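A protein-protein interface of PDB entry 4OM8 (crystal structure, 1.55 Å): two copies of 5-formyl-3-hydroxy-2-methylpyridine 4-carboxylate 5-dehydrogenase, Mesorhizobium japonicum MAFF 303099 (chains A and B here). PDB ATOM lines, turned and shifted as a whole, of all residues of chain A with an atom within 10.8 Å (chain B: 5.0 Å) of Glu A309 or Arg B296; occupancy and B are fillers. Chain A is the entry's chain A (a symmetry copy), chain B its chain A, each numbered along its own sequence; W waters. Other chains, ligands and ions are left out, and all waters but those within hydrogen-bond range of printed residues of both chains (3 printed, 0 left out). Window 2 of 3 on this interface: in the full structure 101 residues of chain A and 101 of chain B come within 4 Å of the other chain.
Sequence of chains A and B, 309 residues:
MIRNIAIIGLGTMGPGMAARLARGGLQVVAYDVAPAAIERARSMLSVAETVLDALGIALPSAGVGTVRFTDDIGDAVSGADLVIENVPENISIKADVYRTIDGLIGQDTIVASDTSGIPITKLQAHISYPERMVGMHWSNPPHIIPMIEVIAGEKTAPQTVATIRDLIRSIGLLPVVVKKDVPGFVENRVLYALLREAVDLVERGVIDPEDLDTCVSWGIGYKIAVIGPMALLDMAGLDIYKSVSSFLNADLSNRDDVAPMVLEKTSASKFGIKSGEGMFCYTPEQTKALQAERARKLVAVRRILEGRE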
ATOM      1  N   ALA A  54     -18.904  31.958  25.927  1.00  0.00           N
ATOM      2  CA  ALA A  54     -18.639  30.996  24.867  1.00  0.00           C
ATOM      3  C   ALA A  54     -17.558  30.008  25.287  1.00  0.00           C
ATOM      4  O   ALA A  54     -17.526  28.880  24.804  1.00  0.00           O
ATOM      5  CB  ALA A  54     -18.242  31.716  23.595  1.00  0.00           C
ATOM      6  N   LEU A  55     -16.661  30.437  26.173  1.00  0.00           N
ATOM      7  CA  LEU A  55     -15.640  29.541  26.707  1.00  0.00           C
ATOM      8  C   LEU A  55     -16.161  28.653  27.831  1.00  0.00           C
ATOM      9  O   LEU A  55     -15.452  27.766  28.313  1.00  0.00           O
ATOM     10  CB  LEU A  55     -14.446  30.355  27.210  1.00  0.00           C
ATOM     11  CG  LEU A  55     -13.529  30.897  26.114  1.00  0.00           C
ATOM     12  CD1 LEU A  55     -12.586  31.934  26.689  1.00  0.00           C
ATOM     13  CD2 LEU A  55     -12.741  29.751  25.447  1.00  0.00           C
ATOM     14  N   TYR A 222       0.064  23.703  15.324  1.00  0.00           N
ATOM     15  CA  TYR A 222      -1.013  22.729  15.448  1.00  0.00           C
ATOM     16  C   TYR A 222      -0.605  21.576  16.362  1.00  0.00           C
ATOM     17  O   TYR A 222      -1.332  21.218  17.293  1.00  0.00           O
ATOM     18  CB  TYR A 222      -1.383  22.259  14.038  1.00  0.00           C
ATOM     19  CG  TYR A 222      -2.262  21.043  13.876  1.00  0.00           C
ATOM     20  CD1 TYR A 222      -3.476  20.922  14.535  1.00  0.00           C
ATOM     21  CD2 TYR A 222      -1.898  20.049  12.979  1.00  0.00           C
ATOM     22  CE1 TYR A 222      -4.286  19.811  14.325  1.00  0.00           C
ATOM     23  CE2 TYR A 222      -2.686  18.955  12.762  1.00  0.00           C
ATOM     24  CZ  TYR A 222      -3.873  18.829  13.439  1.00  0.00           C
ATOM     25  OH  TYR A 222      -4.651  17.710  13.199  1.00  0.00           O
ATOM     26  N   VAL A 226      -1.304  20.767  21.040  1.00  0.00           N
ATOM     27  CA  VAL A 226      -1.749  19.516  21.649  1.00  0.00           C
ATOM     28  C   VAL A 226      -0.653  18.854  22.484  1.00  0.00           C
ATOM     29  O   VAL A 226      -0.922  18.241  23.522  1.00  0.00           O
ATOM     30  CB  VAL A 226      -2.220  18.542  20.548  1.00  0.00           C
ATOM     31  CG1 VAL A 226      -2.645  17.216  21.138  1.00  0.00           C
ATOM     32  CG2 VAL A 226      -3.377  19.164  19.760  1.00  0.00           C
ATOM     33  N   ILE A 227       0.587  18.984  22.023  1.00  0.00           N
ATOM     34  CA  ILE A 227       1.729  18.314  22.625  1.00  0.00           C
ATOM     35  C   ILE A 227       2.865  19.314  22.850  1.00  0.00           C
ATOM     36  O   ILE A 227       3.492  19.731  21.892  1.00  0.00           O
ATOM     37  CB  ILE A 227       2.250  17.176  21.719  1.00  0.00           C
ATOM     38  CG1 ILE A 227       1.113  16.226  21.323  1.00  0.00           C
ATOM     39  CG2 ILE A 227       3.369  16.411  22.430  1.00  0.00           C
ATOM     40  CD1 ILE A 227       1.381  15.477  20.027  1.00  0.00           C
ATOM     41  N   ALA A 300     -12.891  28.113  19.810  1.00  0.00           N
ATOM     42  CA  ALA A 300     -13.284  26.731  19.521  1.00  0.00           C
ATOM     43  C   ALA A 300     -12.133  25.753  19.779  1.00  0.00           C
ATOM     44  O   ALA A 300     -12.334  24.662  20.328  1.00  0.00           O
ATOM     45  CB  ALA A 300     -13.773  26.610  18.091  1.00  0.00           C
ATOM     46  N   VAL A 301     -10.931  26.148  19.376  1.00  0.00           N
ATOM     47  CA  VAL A 301      -9.758  25.303  19.557  1.00  0.00           C
ATOM     48  C   VAL A 301      -9.453  25.120  21.043  1.00  0.00           C
ATOM     49  O   VAL A 301      -9.154  24.018  21.500  1.00  0.00           O
ATOM     50  CB  VAL A 301      -8.535  25.902  18.830  1.00  0.00           C
ATOM     51  CG1 VAL A 301      -7.239  25.230  19.297  1.00  0.00           C
ATOM     52  CG2 VAL A 301      -8.713  25.772  17.316  1.00  0.00           C
ATOM     53  N   ARG A 302      -9.556  26.198  21.816  1.00  0.00           N
ATOM     54  CA  ARG A 302      -9.251  26.093  23.235  1.00  0.00           C
ATOM     55  C   ARG A 302     -10.139  25.062  23.928  1.00  0.00           C
ATOM     56  O   ARG A 302      -9.654  24.266  24.739  1.00  0.00           O
ATOM     57  CB  ARG A 302      -9.386  27.455  23.926  1.00  0.00           C
ATOM     58  CG  ARG A 302      -9.450  27.312  25.432  1.00  0.00           C
ATOM     59  CD  ARG A 302      -9.255  28.613  26.184  1.00  0.00           C
ATOM     60  NE  ARG A 302      -9.564  28.381  27.592  1.00  0.00           N
ATOM     61  CZ  ARG A 302      -9.621  29.324  28.530  1.00  0.00           C
ATOM     62  NH1 ARG A 302      -9.386  30.596  28.230  1.00  0.00           N
ATOM     63  NH2 ARG A 302      -9.924  28.979  29.771  1.00  0.00           N
ATOM     64  N   ARG A 303     -11.428  25.049  23.596  1.00  0.00           N
ATOM     65  CA  ARG A 303     -12.328  24.104  24.238  1.00  0.00           C
ATOM     66  C   ARG A 303     -11.912  22.670  23.932  1.00  0.00           C
ATOM     67  O   ARG A 303     -11.959  21.809  24.808  1.00  0.00           O
ATOM     68  CB  ARG A 303     -13.768  24.372  23.816  1.00  0.00           C
ATOM     69  CG  ARG A 303     -14.223  25.751  24.261  1.00  0.00           C
ATOM     70  CD  ARG A 303     -15.718  25.830  24.357  1.00  0.00           C
ATOM     71  NE  ARG A 303     -16.363  25.423  23.118  1.00  0.00           N
ATOM     72  CZ  ARG A 303     -17.677  25.300  22.977  1.00  0.00           C
ATOM     73  NH1 ARG A 303     -18.476  25.552  24.002  1.00  0.00           N
ATOM     74  NH2 ARG A 303     -18.194  24.930  21.815  1.00  0.00           N
ATOM     75  N   ILE A 304     -11.474  22.413  22.704  1.00  0.00           N
ATOM     76  CA  ILE A 304     -10.972  21.080  22.378  1.00  0.00           C
ATOM     77  C   ILE A 304      -9.706  20.729  23.173  1.00  0.00           C
ATOM     78  O   ILE A 304      -9.567  19.624  23.687  1.00  0.00           O
ATOM     79  CB  ILE A 304     -10.665  20.941  20.878  1.00  0.00           C
ATOM     80  CG1 ILE A 304     -11.921  21.211  20.051  1.00  0.00           C
ATOM     81  CG2 ILE A 304     -10.046  19.570  20.599  1.00  0.00           C
ATOM     82  CD1 ILE A 304     -13.061  20.356  20.443  1.00  0.00           C
ATOM     83  N   LEU A 305      -8.790  21.684  23.280  1.00  0.00           N
ATOM     84  CA  LEU A 305      -7.517  21.436  23.948  1.00  0.00           C
ATOM     85  C   LEU A 305      -7.715  21.162  25.429  1.00  0.00           C
ATOM     86  O   LEU A 305      -6.910  20.457  26.055  1.00  0.00           O
ATOM     87  CB  LEU A 305      -6.575  22.624  23.753  1.00  0.00           C
ATOM     88  CG  LEU A 305      -6.050  22.859  22.340  1.00  0.00           C
ATOM     89  CD1 LEU A 305      -5.171  24.079  22.297  1.00  0.00           C
ATOM     90  CD2 LEU A 305      -5.293  21.643  21.820  1.00  0.00           C
ATOM     91  N   GLU A 306      -8.794  21.721  25.973  1.00  0.00           N
ATOM     92  CA  GLU A 306      -9.160  21.529  27.374  1.00  0.00           C
ATOM     93  C   GLU A 306      -9.886  20.219  27.631  1.00  0.00           C
ATOM     94  O   GLU A 306     -10.210  19.901  28.777  1.00  0.00           O
ATOM     95  CB  GLU A 306     -10.037  22.682  27.844  1.00  0.00           C
ATOM     96  CG  GLU A 306      -9.302  23.970  27.932  1.00  0.00           C
ATOM     97  CD  GLU A 306     -10.212  25.130  28.288  1.00  0.00           C
ATOM     98  OE1 GLU A 306     -11.434  25.077  27.990  1.00  0.00           O
ATOM     99  OE2 GLU A 306      -9.694  26.098  28.856  1.00  0.00           O
ATOM    100  N   GLY A 307     -10.173  19.482  26.563  1.00  0.00           N
ATOM    101  CA  GLY A 307     -10.793  18.173  26.678  1.00  0.00           C
ATOM    102  C   GLY A 307     -12.300  18.163  26.512  1.00  0.00           C
ATOM    103  O   GLY A 307     -12.948  17.149  26.787  1.00  0.00           O
ATOM    104  N   ARG A 308     -12.865  19.281  26.068  1.00  0.00           N
ATOM    105  CA  ARG A 308     -14.318  19.385  25.971  1.00  0.00           C
ATOM    106  C   ARG A 308     -14.859  18.472  24.887  1.00  0.00           C
ATOM    107  O   ARG A 308     -14.269  18.338  23.814  1.00  0.00           O
ATOM    108  CB  ARG A 308     -14.757  20.822  25.695  1.00  0.00           C
ATOM    109  CG  ARG A 308     -16.261  21.003  25.735  1.00  0.00           C
ATOM    110  CD  ARG A 308     -16.670  22.383  25.270  1.00  0.00           C
ATOM    111  NE  ARG A 308     -18.046  22.691  25.650  1.00  0.00           N
ATOM    112  CZ  ARG A 308     -19.092  22.558  24.839  1.00  0.00           C
ATOM    113  NH1 ARG A 308     -18.925  22.111  23.599  1.00  0.00           N
ATOM    114  NH2 ARG A 308     -20.310  22.869  25.270  1.00  0.00           N
ATOM    115  N   GLU A 309     -15.994  17.850  25.189  1.00  0.00           N
ATOM    116  CA  GLU A 309     -16.706  17.008  24.235  1.00  0.00           C
ATOM    117  C   GLU A 309     -18.121  17.546  24.062  1.00  0.00           C
ATOM    118  O   GLU A 309     -19.106  16.954  24.529  1.00  0.00           O
ATOM    119  CB  GLU A 309     -16.721  15.546  24.699  1.00  0.00           C
ATOM    120  CG  GLU A 309     -15.389  14.802  24.516  1.00  0.00           C
ATOM    121  CD  GLU A 309     -15.163  14.335  23.086  1.00  0.00           C
ATOM    122  OE1 GLU A 309     -15.721  14.958  22.158  1.00  0.00           O
ATOM    123  OE2 GLU A 309     -14.432  13.334  22.885  1.00  0.00           O
ATOM    124  OXT GLU A 309     -18.281  18.613  23.453  1.00  0.00           O
ATOM    125  N   ALA B 292      -4.103   7.973  22.249  1.00  0.00           N
ATOM    126  CA  ALA B 292      -5.480   8.069  21.775  1.00  0.00           C
ATOM    127  C   ALA B 292      -5.996   9.499  21.895  1.00  0.00           C
ATOM    128  O   ALA B 292      -6.644  10.023  20.981  1.00  0.00           O
ATOM    129  CB  ALA B 292      -6.382   7.113  22.555  1.00  0.00           C
ATOM    130  N   GLU B 293      -5.706  10.125  23.026  1.00  0.00           N
ATOM    131  CA  GLU B 293      -6.223  11.458  23.283  1.00  0.00           C
ATOM    132  C   GLU B 293      -5.552  12.494  22.385  1.00  0.00           C
ATOM    133  O   GLU B 293      -6.201  13.438  21.924  1.00  0.00           O
ATOM    134  CB  GLU B 293      -6.052  11.827  24.752  1.00  0.00           C
ATOM    135  CG  GLU B 293      -6.719  13.128  25.124  1.00  0.00           C
ATOM    136  CD  GLU B 293      -8.261  13.074  25.140  1.00  0.00           C
ATOM    137  OE1 GLU B 293      -8.889  12.093  24.664  1.00  0.00           O
ATOM    138  OE2 GLU B 293      -8.848  14.047  25.649  1.00  0.00           O
ATOM    139  N   ARG B 294      -4.263  12.315  22.101  1.00  0.00           N
ATOM    140  CA  ARG B 294      -3.601  13.239  21.195  1.00  0.00           C
ATOM    141  C   ARG B 294      -4.148  13.110  19.778  1.00  0.00           C
ATOM    142  O   ARG B 294      -4.378  14.122  19.106  1.00  0.00           O
ATOM    143  CB  ARG B 294      -2.083  13.022  21.220  1.00  0.00           C
ATOM    144  CG  ARG B 294      -1.461  13.493  22.537  1.00  0.00           C
ATOM    145  CD  ARG B 294      -0.053  12.914  22.737  1.00  0.00           C
ATOM    146  NE  ARG B 294       0.590  13.533  23.886  1.00  0.00           N
ATOM    147  CZ  ARG B 294       1.784  13.189  24.370  1.00  0.00           C
ATOM    148  NH1 ARG B 294       2.458  12.187  23.828  1.00  0.00           N
ATOM    149  NH2 ARG B 294       2.283  13.831  25.422  1.00  0.00           N
ATOM    150  N   ALA B 295      -4.384  11.882  19.321  1.00  0.00           N
ATOM    151  CA  ALA B 295      -4.950  11.706  17.984  1.00  0.00           C
ATOM    152  C   ALA B 295      -6.350  12.309  17.903  1.00  0.00           C
ATOM    153  O   ALA B 295      -6.717  12.932  16.900  1.00  0.00           O
ATOM    154  CB  ALA B 295      -4.991  10.231  17.601  1.00  0.00           C
ATOM    155  N   ARG B 296      -7.124  12.139  18.969  1.00  0.00           N
ATOM    156  CA  ARG B 296      -8.486  12.664  18.982  1.00  0.00           C
ATOM    157  C   ARG B 296      -8.502  14.189  18.955  1.00  0.00           C
ATOM    158  O   ARG B 296      -9.240  14.798  18.183  1.00  0.00           O
ATOM    159  CB  ARG B 296      -9.246  12.169  20.209  1.00  0.00           C
ATOM    160  CG  ARG B 296     -10.700  12.617  20.209  1.00  0.00           C
ATOM    161  CD  ARG B 296     -11.360  12.327  21.537  1.00  0.00           C
ATOM    162  NE  ARG B 296     -10.831  13.163  22.606  1.00  0.00           N
ATOM    163  CZ  ARG B 296     -11.088  14.458  22.740  1.00  0.00           C
ATOM    164  NH1 ARG B 296     -11.868  15.076  21.860  1.00  0.00           N
ATOM    165  NH2 ARG B 296     -10.565  15.133  23.750  1.00  0.00           N
ATOM    166  N   LYS B 297      -7.685  14.807  19.802  1.00  0.00           N
ATOM    167  CA  LYS B 297      -7.562  16.265  19.797  1.00  0.00           C
ATOM    168  C   LYS B 297      -7.032  16.818  18.467  1.00  0.00           C
ATOM    169  O   LYS B 297      -7.532  17.832  17.978  1.00  0.00           O
ATOM    170  CB  LYS B 297      -6.652  16.730  20.934  1.00  0.00           C
ATOM    171  CG  LYS B 297      -7.268  16.634  22.321  1.00  0.00           C
ATOM    172  CD  LYS B 297      -6.230  17.011  23.357  1.00  0.00           C
ATOM    173  CE  LYS B 297      -6.771  17.013  24.759  1.00  0.00           C
ATOM    174  NZ  LYS B 297      -5.621  17.198  25.692  1.00  0.00           N
ATOM    175  N   LEU B 298      -6.018  16.167  17.889  1.00  0.00           N
ATOM    176  CA  LEU B 298      -5.502  16.619  16.596  1.00  0.00           C
ATOM    177  C   LEU B 298      -6.596  16.637  15.543  1.00  0.00           C
ATOM    178  O   LEU B 298      -6.721  17.606  14.780  1.00  0.00           O
ATOM    179  CB  LEU B 298      -4.342  15.736  16.125  1.00  0.00           C
ATOM    180  CG  LEU B 298      -3.005  15.955  16.844  1.00  0.00           C
ATOM    181  CD1 LEU B 298      -2.024  14.871  16.435  1.00  0.00           C
ATOM    182  CD2 LEU B 298      -2.431  17.346  16.550  1.00  0.00           C
ATOM    183  N   VAL B 299      -7.405  15.582  15.498  1.00  0.00           N
ATOM    184  CA  VAL B 299      -8.469  15.549  14.505  1.00  0.00           C
ATOM    185  C   VAL B 299      -9.488  16.673  14.752  1.00  0.00           C
ATOM    186  O   VAL B 299      -9.854  17.392  13.819  1.00  0.00           O
ATOM    187  CB  VAL B 299      -9.158  14.166  14.469  1.00  0.00           C
ATOM    188  CG1 VAL B 299     -10.460  14.241  13.683  1.00  0.00           C
ATOM    189  CG2 VAL B 299      -8.201  13.148  13.849  1.00  0.00           C
ATOM    190  N   ALA B 300      -9.913  16.857  16.002  1.00  0.00           N
ATOM    191  CA  ALA B 300     -10.939  17.862  16.299  1.00  0.00           C
ATOM    192  C   ALA B 300     -10.430  19.281  16.032  1.00  0.00           C
ATOM    193  O   ALA B 300     -11.152  20.127  15.487  1.00  0.00           O
ATOM    194  CB  ALA B 300     -11.409  17.727  17.734  1.00  0.00           C
HETATM  195  O   HOH W   1     -11.568  17.803  23.439  1.00  0.00           O
HETATM  196  O   HOH W   2      -3.480  19.024  24.597  1.00  0.00           O
HETATM  197  O   HOH W   3      -0.934  15.855  24.804  1.00  0.00           O
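The guanidinium group (NH1) of Arg B296 is in salt-bridge range of the side-chain carboxylate (OE2) of Glu A309.
The side-chain hydroxyl (OH) of Tyr A222 sits at hydrogen-bond distance from the backbone carbonyl oxygen (O) of Leu B298.
Glu A309 touches one residue of chain B.
Arg B296 touches one residue of chain A.
No residue of chain A comes within 4 Å of Glu B293.
Printed residues of chain A within 4 Å of Lys B297: Ile A304 and Leu A305.
Val B299 touches none of the printed residues of chain A.
Ala B300 touches just one residue of chain A: Ile A304.
Of the printed residues of chain A, Arg B294 touches Ile A227 (3.8 Å).
Printed residues of chain B within 4 Å of Ile A304: Lys B297 and Ala B300.
Of the printed residues of chain B, Tyr A222 touches Leu B298 (2.6 Å).
Printed residues of chain A within 4 Å of Leu B298: Tyr A222 (2.6 Å) and Val A226 (3.8 Å).
Arg A302 touches none of the printed residues of chain B.
The nearest printed residue of chain B that does not touch Glu A309 is Glu B293 (6.0 Å).
The nearest printed residue of chain A that does not touch Leu B298 is Ile A227 (5.0 Å).
NH2 of Arg B296 lies within salt-bridge range of OE2 of Glu B293 (2.8 Å).
Among the printed residues, pairs that only touch across the chains: Leu A305 with Lys B297 (3.5 Å), Ile A304 with Ala B300 (3.7 Å), Ile A227 with Arg B294 (3.8 Å), Val A226 with Leu B298 (3.8 Å) and Ile A304 with Lys B297 (3.97 Å).
Hydrophobic or aromatic side chains of chain A that line the printed part of chain B: Tyr A222, Val A226, Ile A227 and Ile A304.
Along chain A the printed residues that touch a printed residue of chain B span positions 222 to 309.
Among the printed residues, 7 pairs touch across the chains.
Among the printed residues, Asp or Glu carboxylates within 4 Å of a Lys or Arg side-chain nitrogen of the other chain: Glu A309 with Arg B296 (3.3 Å).
Water W3 bridges O of Val A226 and NE of Arg B294.
Water W1 lies within hydrogen-bond range of O of Ile A304 (2.7 Å), O of Arg A308 (2.8 Å) and NH2 of Arg B296 (2.9 Å).
Water W2 bridges O of Val A226 (2.9 Å) and NZ of Lys B297 (3.0 Å).
1 position is printed for both chains.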
